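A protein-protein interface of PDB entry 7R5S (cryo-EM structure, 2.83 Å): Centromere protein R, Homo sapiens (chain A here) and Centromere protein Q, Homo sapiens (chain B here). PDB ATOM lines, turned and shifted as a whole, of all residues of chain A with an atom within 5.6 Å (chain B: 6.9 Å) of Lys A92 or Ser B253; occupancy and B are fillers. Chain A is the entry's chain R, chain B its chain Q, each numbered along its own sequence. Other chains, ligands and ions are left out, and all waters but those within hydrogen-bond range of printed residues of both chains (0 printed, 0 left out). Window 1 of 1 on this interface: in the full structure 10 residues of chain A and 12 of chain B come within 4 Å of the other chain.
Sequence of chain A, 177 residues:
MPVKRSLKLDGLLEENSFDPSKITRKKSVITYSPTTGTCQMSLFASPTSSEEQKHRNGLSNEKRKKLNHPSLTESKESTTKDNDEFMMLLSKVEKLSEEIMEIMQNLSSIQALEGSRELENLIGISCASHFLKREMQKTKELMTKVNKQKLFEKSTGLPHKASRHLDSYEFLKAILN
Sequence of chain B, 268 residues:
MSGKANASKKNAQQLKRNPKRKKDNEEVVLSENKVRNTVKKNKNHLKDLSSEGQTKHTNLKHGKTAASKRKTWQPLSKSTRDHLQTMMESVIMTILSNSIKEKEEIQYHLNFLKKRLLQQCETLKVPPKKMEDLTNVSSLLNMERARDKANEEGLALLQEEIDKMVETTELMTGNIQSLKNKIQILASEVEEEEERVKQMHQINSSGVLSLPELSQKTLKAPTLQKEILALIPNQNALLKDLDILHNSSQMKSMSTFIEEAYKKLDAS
The backbone carbonyl oxygen of Ser B253 sits at hydrogen-bond distance from the side-chain hydroxyl of Thr B256 (2.5 Å).
The side-chain hydroxyl of Ser B253 is in hydrogen-bond range of the backbone carbonyl oxygen of Gln B250 (2.6 Å).
The backbone carbonyl oxygen (O) of Ser B249 sits at hydrogen-bond distance from the side-chain hydroxyl (OG) of Ser B253 (2.9 Å).
Leu A89 touches Phe B257 (CD1 to CD1, 3.6 Å).
NZ of Lys A92 touches CB of Ser B253, at 3.7 Å.
CD1 of Leu A96 touches CG of Gln B250, 3.6 Å away.
Ser B253 touches Leu A96.
Lys A92 touches just one residue of chain B: Ser B253 (3.7 Å).
Printed residues of chain A within 4 Å of Ser B253: Lys A92 and Leu A96.
Printed residues of chain A within 4 Å of Gln B250: Leu A96.
Printed residues of chain A within 4 Å of Phe B257: Leu A89 (3.6 Å).
Of the printed residues of chain B, Leu A89 touches Phe B257 (3.6 Å).
Of the printed residues of chain B, Leu A96 touches Gln B250 and Ser B253.
The nearest residue of chain B that does not touch Lys A92 is Thr B256 (4.6 Å).
The nearest printed residue of chain B that does not touch Leu A89 is Thr B256 (7.2 Å).
Printed residues of chain A that touch a printed residue of chain B: Leu A89, Lys A92 and Leu A96.
Hydrophobic or aromatic side chains of chain A that line the printed part of chain B: Leu A89 and Leu A96.
Of the 11 printed residues of chain B, 3 touch a printed residue of chain A.
Printed residues of chain B that touch a printed residue of chain A: Gln B250, Ser B253 and Phe B257.
Hydrophobic or aromatic side chains of chain B that line the printed part of chain A: Phe B257.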
ATOM      1  N   MET A  87     -33.445   7.630 -29.095  1.00  0.00           N
ATOM      2  CA  MET A  87     -33.678   7.491 -27.662  1.00  0.00           C
ATOM      3  C   MET A  87     -32.363   7.370 -26.899  1.00  0.00           C
ATOM      4  O   MET A  87     -32.122   8.094 -25.927  1.00  0.00           O
ATOM      5  CB  MET A  87     -34.570   6.277 -27.394  1.00  0.00           C
ATOM      6  CG  MET A  87     -35.727   6.115 -28.369  1.00  0.00           C
ATOM      7  SD  MET A  87     -36.480   7.686 -28.831  1.00  0.00           S
ATOM      8  CE  MET A  87     -37.602   7.931 -27.456  1.00  0.00           C
ATOM      9  N   MET A  88     -31.491   6.459 -27.337  1.00  0.00           N
ATOM     10  CA  MET A  88     -30.249   6.231 -26.608  1.00  0.00           C
ATOM     11  C   MET A  88     -29.249   7.367 -26.787  1.00  0.00           C
ATOM     12  O   MET A  88     -28.510   7.670 -25.843  1.00  0.00           O
ATOM     13  CB  MET A  88     -29.624   4.893 -27.019  1.00  0.00           C
ATOM     14  CG  MET A  88     -29.403   4.691 -28.509  1.00  0.00           C
ATOM     15  SD  MET A  88     -27.890   5.459 -29.120  1.00  0.00           S
ATOM     16  CE  MET A  88     -26.667   4.635 -28.102  1.00  0.00           C
ATOM     17  N   LEU A  89     -29.208   8.019 -27.955  1.00  0.00           N
ATOM     18  CA  LEU A  89     -28.313   9.165 -28.086  1.00  0.00           C
ATOM     19  C   LEU A  89     -28.774  10.317 -27.199  1.00  0.00           C
ATOM     20  O   LEU A  89     -27.950  10.993 -26.569  1.00  0.00           O
ATOM     21  CB  LEU A  89     -28.191   9.604 -29.549  1.00  0.00           C
ATOM     22  CG  LEU A  89     -29.317  10.294 -30.323  1.00  0.00           C
ATOM     23  CD1 LEU A  89     -29.314  11.803 -30.116  1.00  0.00           C
ATOM     24  CD2 LEU A  89     -29.181   9.973 -31.800  1.00  0.00           C
ATOM     25  N   LEU A  90     -30.089  10.536 -27.108  1.00  0.00           N
ATOM     26  CA  LEU A  90     -30.609  11.515 -26.160  1.00  0.00           C
ATOM     27  C   LEU A  90     -30.281  11.135 -24.725  1.00  0.00           C
ATOM     28  O   LEU A  90     -29.908  12.000 -23.924  1.00  0.00           O
ATOM     29  CB  LEU A  90     -32.121  11.651 -26.315  1.00  0.00           C
ATOM     30  CG  LEU A  90     -32.731  12.902 -25.692  1.00  0.00           C
ATOM     31  CD1 LEU A  90     -32.549  14.126 -26.587  1.00  0.00           C
ATOM     32  CD2 LEU A  90     -34.187  12.648 -25.353  1.00  0.00           C
ATOM     33  N   SER A  91     -30.415   9.854 -24.382  1.00  0.00           N
ATOM     34  CA  SER A  91     -30.109   9.420 -23.026  1.00  0.00           C
ATOM     35  C   SER A  91     -28.650   9.696 -22.685  1.00  0.00           C
ATOM     36  O   SER A  91     -28.341  10.239 -21.616  1.00  0.00           O
ATOM     37  CB  SER A  91     -30.431   7.934 -22.865  1.00  0.00           C
ATOM     38  OG  SER A  91     -31.684   7.621 -23.447  1.00  0.00           O
ATOM     39  N   LYS A  92     -27.737   9.351 -23.598  1.00  0.00           N
ATOM     40  CA  LYS A  92     -26.322   9.533 -23.299  1.00  0.00           C
ATOM     41  C   LYS A  92     -25.935  11.007 -23.269  1.00  0.00           C
ATOM     42  O   LYS A  92     -25.092  11.397 -22.456  1.00  0.00           O
ATOM     43  CB  LYS A  92     -25.448   8.755 -24.290  1.00  0.00           C
ATOM     44  CG  LYS A  92     -25.635   9.089 -25.756  1.00  0.00           C
ATOM     45  CD  LYS A  92     -24.591  10.085 -26.236  1.00  0.00           C
ATOM     46  CE  LYS A  92     -24.763  10.403 -27.713  1.00  0.00           C
ATOM     47  NZ  LYS A  92     -23.690  11.311 -28.208  1.00  0.00           N
ATOM     48  N   VAL A  93     -26.547  11.853 -24.107  1.00  0.00           N
ATOM     49  CA  VAL A  93     -26.204  13.271 -24.009  1.00  0.00           C
ATOM     50  C   VAL A  93     -26.788  13.872 -22.733  1.00  0.00           C
ATOM     51  O   VAL A  93     -26.193  14.782 -22.140  1.00  0.00           O
ATOM     52  CB  VAL A  93     -26.652  14.060 -25.257  1.00  0.00           C
ATOM     53  CG1 VAL A  93     -25.888  13.599 -26.494  1.00  0.00           C
ATOM     54  CG2 VAL A  93     -28.148  13.987 -25.461  1.00  0.00           C
ATOM     55  N   GLU A  94     -27.927  13.358 -22.260  1.00  0.00           N
ATOM     56  CA  GLU A  94     -28.454  13.826 -20.983  1.00  0.00           C
ATOM     57  C   GLU A  94     -27.552  13.427 -19.822  1.00  0.00           C
ATOM     58  O   GLU A  94     -27.310  14.239 -18.922  1.00  0.00           O
ATOM     59  CB  GLU A  94     -29.867  13.287 -20.764  1.00  0.00           C
ATOM     60  CG  GLU A  94     -30.604  13.883 -19.565  1.00  0.00           C
ATOM     61  CD  GLU A  94     -30.504  15.398 -19.482  1.00  0.00           C
ATOM     62  OE1 GLU A  94     -29.511  15.908 -18.921  1.00  0.00           O
ATOM     63  OE2 GLU A  94     -31.429  16.083 -19.965  1.00  0.00           O
ATOM     64  N   LYS A  95     -27.039  12.194 -19.826  1.00  0.00           N
ATOM     65  CA  LYS A  95     -26.065  11.815 -18.803  1.00  0.00           C
ATOM     66  C   LYS A  95     -24.792  12.645 -18.926  1.00  0.00           C
ATOM     67  O   LYS A  95     -24.163  12.986 -17.918  1.00  0.00           O
ATOM     68  CB  LYS A  95     -25.739  10.321 -18.883  1.00  0.00           C
ATOM     69  CG  LYS A  95     -26.926   9.406 -19.127  1.00  0.00           C
ATOM     70  CD  LYS A  95     -28.013   9.581 -18.075  1.00  0.00           C
ATOM     71  CE  LYS A  95     -29.338   9.005 -18.556  1.00  0.00           C
ATOM     72  NZ  LYS A  95     -30.239  10.040 -19.136  1.00  0.00           N
ATOM     73  N   LEU A  96     -24.404  12.987 -20.156  1.00  0.00           N
ATOM     74  CA  LEU A  96     -23.185  13.748 -20.390  1.00  0.00           C
ATOM     75  C   LEU A  96     -23.344  15.221 -20.026  1.00  0.00           C
ATOM     76  O   LEU A  96     -22.339  15.933 -19.918  1.00  0.00           O
ATOM     77  CB  LEU A  96     -22.784  13.609 -21.859  1.00  0.00           C
ATOM     78  CG  LEU A  96     -21.342  13.899 -22.262  1.00  0.00           C
ATOM     79  CD1 LEU A  96     -20.405  12.993 -21.495  1.00  0.00           C
ATOM     80  CD2 LEU A  96     -21.169  13.703 -23.749  1.00  0.00           C
ATOM     81  N   SER A  97     -24.587  15.690 -19.879  1.00  0.00           N
ATOM     82  CA  SER A  97     -24.839  17.087 -19.529  1.00  0.00           C
ATOM     83  C   SER A  97     -24.162  17.473 -18.217  1.00  0.00           C
ATOM     84  O   SER A  97     -23.575  18.554 -18.098  1.00  0.00           O
ATOM     85  CB  SER A  97     -26.346  17.341 -19.452  1.00  0.00           C
ATOM     86  OG  SER A  97     -26.844  17.082 -18.151  1.00  0.00           O
ATOM     87  N   SER B 248     -11.406  17.202 -25.629  1.00  0.00           N
ATOM     88  CA  SER B 248     -12.413  16.457 -24.885  1.00  0.00           C
ATOM     89  C   SER B 248     -13.507  15.966 -25.824  1.00  0.00           C
ATOM     90  O   SER B 248     -14.021  16.727 -26.648  1.00  0.00           O
ATOM     91  CB  SER B 248     -13.008  17.327 -23.778  1.00  0.00           C
ATOM     92  OG  SER B 248     -11.995  18.024 -23.073  1.00  0.00           O
ATOM     93  N   SER B 249     -13.860  14.685 -25.699  1.00  0.00           N
ATOM     94  CA  SER B 249     -14.863  14.068 -26.560  1.00  0.00           C
ATOM     95  C   SER B 249     -16.291  14.374 -26.130  1.00  0.00           C
ATOM     96  O   SER B 249     -17.220  14.115 -26.903  1.00  0.00           O
ATOM     97  CB  SER B 249     -14.657  12.551 -26.601  1.00  0.00           C
ATOM     98  OG  SER B 249     -14.977  11.959 -25.355  1.00  0.00           O
ATOM     99  N   GLN B 250     -16.489  14.911 -24.925  1.00  0.00           N
ATOM    100  CA  GLN B 250     -17.831  15.283 -24.488  1.00  0.00           C
ATOM    101  C   GLN B 250     -18.416  16.361 -25.391  1.00  0.00           C
ATOM    102  O   GLN B 250     -19.525  16.213 -25.922  1.00  0.00           O
ATOM    103  CB  GLN B 250     -17.794  15.758 -23.035  1.00  0.00           C
ATOM    104  CG  GLN B 250     -17.318  14.716 -22.039  1.00  0.00           C
ATOM    105  CD  GLN B 250     -15.809  14.685 -21.901  1.00  0.00           C
ATOM    106  OE1 GLN B 250     -15.083  15.049 -22.825  1.00  0.00           O
ATOM    107  NE2 GLN B 250     -15.329  14.247 -20.744  1.00  0.00           N
ATOM    108  N   MET B 251     -17.675  17.454 -25.587  1.00  0.00           N
ATOM    109  CA  MET B 251     -18.119  18.486 -26.510  1.00  0.00           C
ATOM    110  C   MET B 251     -18.189  17.981 -27.944  1.00  0.00           C
ATOM    111  O   MET B 251     -19.030  18.455 -28.712  1.00  0.00           O
ATOM    112  CB  MET B 251     -17.199  19.706 -26.435  1.00  0.00           C
ATOM    113  CG  MET B 251     -17.570  20.801 -27.421  1.00  0.00           C
ATOM    114  SD  MET B 251     -19.339  21.163 -27.441  1.00  0.00           S
ATOM    115  CE  MET B 251     -19.521  21.837 -29.090  1.00  0.00           C
ATOM    116  N   LYS B 252     -17.351  17.018 -28.321  1.00  0.00           N
ATOM    117  CA  LYS B 252     -17.436  16.473 -29.673  1.00  0.00           C
ATOM    118  C   LYS B 252     -18.755  15.743 -29.883  1.00  0.00           C
ATOM    119  O   LYS B 252     -19.427  15.936 -30.902  1.00  0.00           O
ATOM    120  CB  LYS B 252     -16.246  15.554 -29.952  1.00  0.00           C
ATOM    121  CG  LYS B 252     -14.883  16.208 -29.749  1.00  0.00           C
ATOM    122  CD  LYS B 252     -14.915  17.684 -30.129  1.00  0.00           C
ATOM    123  CE  LYS B 252     -13.793  18.459 -29.475  1.00  0.00           C
ATOM    124  NZ  LYS B 252     -13.743  19.863 -29.971  1.00  0.00           N
ATOM    125  N   SER B 253     -19.156  14.915 -28.918  1.00  0.00           N
ATOM    126  CA  SER B 253     -20.453  14.252 -29.003  1.00  0.00           C
ATOM    127  C   SER B 253     -21.592  15.264 -28.958  1.00  0.00           C
ATOM    128  O   SER B 253     -22.604  15.104 -29.652  1.00  0.00           O
ATOM    129  CB  SER B 253     -20.589  13.229 -27.875  1.00  0.00           C
ATOM    130  OG  SER B 253     -20.062  13.747 -26.669  1.00  0.00           O
ATOM    131  N   MET B 254     -21.443  16.316 -28.149  1.00  0.00           N
ATOM    132  CA  MET B 254     -22.436  17.387 -28.125  1.00  0.00           C
ATOM    133  C   MET B 254     -22.586  18.028 -29.502  1.00  0.00           C
ATOM    134  O   MET B 254     -23.704  18.280 -29.970  1.00  0.00           O
ATOM    135  CB  MET B 254     -22.039  18.433 -27.079  1.00  0.00           C
ATOM    136  CG  MET B 254     -22.964  19.641 -26.982  1.00  0.00           C
ATOM    137  SD  MET B 254     -24.682  19.322 -26.518  1.00  0.00           S
ATOM    138  CE  MET B 254     -24.525  17.936 -25.392  1.00  0.00           C
ATOM    139  N   SER B 255     -21.461  18.301 -30.164  1.00  0.00           N
ATOM    140  CA  SER B 255     -21.499  18.926 -31.481  1.00  0.00           C
ATOM    141  C   SER B 255     -22.074  17.978 -32.524  1.00  0.00           C
ATOM    142  O   SER B 255     -22.769  18.412 -33.448  1.00  0.00           O
ATOM    143  CB  SER B 255     -20.097  19.384 -31.882  1.00  0.00           C
ATOM    144  OG  SER B 255     -19.309  18.291 -32.321  1.00  0.00           O
ATOM    145  N   THR B 256     -21.793  16.679 -32.396  1.00  0.00           N
ATOM    146  CA  THR B 256     -22.412  15.708 -33.295  1.00  0.00           C
ATOM    147  C   THR B 256     -23.922  15.679 -33.109  1.00  0.00           C
ATOM    148  O   THR B 256     -24.669  15.591 -34.087  1.00  0.00           O
ATOM    149  CB  THR B 256     -21.826  14.309 -33.084  1.00  0.00           C
ATOM    150  OG1 THR B 256     -22.143  13.842 -31.765  1.00  0.00           O
ATOM    151  CG2 THR B 256     -20.319  14.299 -33.308  1.00  0.00           C
ATOM    152  N   PHE B 257     -24.390  15.760 -31.860  1.00  0.00           N
ATOM    153  CA  PHE B 257     -25.829  15.826 -31.617  1.00  0.00           C
ATOM    154  C   PHE B 257     -26.432  17.085 -32.228  1.00  0.00           C
ATOM    155  O   PHE B 257     -27.491  17.029 -32.869  1.00  0.00           O
ATOM    156  CB  PHE B 257     -26.112  15.768 -30.116  1.00  0.00           C
ATOM    157  CG  PHE B 257     -27.509  16.188 -29.743  1.00  0.00           C
ATOM    158  CD1 PHE B 257     -28.582  15.339 -29.951  1.00  0.00           C
ATOM    159  CD2 PHE B 257     -27.745  17.432 -29.178  1.00  0.00           C
ATOM    160  CE1 PHE B 257     -29.867  15.723 -29.609  1.00  0.00           C
ATOM    161  CE2 PHE B 257     -29.028  17.822 -28.834  1.00  0.00           C
ATOM    162  CZ  PHE B 257     -30.090  16.965 -29.050  1.00  0.00           C
ATOM    163  N   ILE B 258     -25.765  18.228 -32.044  1.00  0.00           N
ATOM    164  CA  ILE B 258     -26.267  19.487 -32.591  1.00  0.00           C
ATOM    165  C   ILE B 258     -26.352  19.411 -34.111  1.00  0.00           C
ATOM    166  O   ILE B 258     -27.372  19.768 -34.713  1.00  0.00           O
ATOM    167  CB  ILE B 258     -25.387  20.664 -32.132  1.00  0.00           C
ATOM    168  CG1 ILE B 258     -25.588  20.932 -30.639  1.00  0.00           C
ATOM    169  CG2 ILE B 258     -25.696  21.912 -32.943  1.00  0.00           C
ATOM    170  CD1 ILE B 258     -24.725  22.050 -30.097  1.00  0.00           C
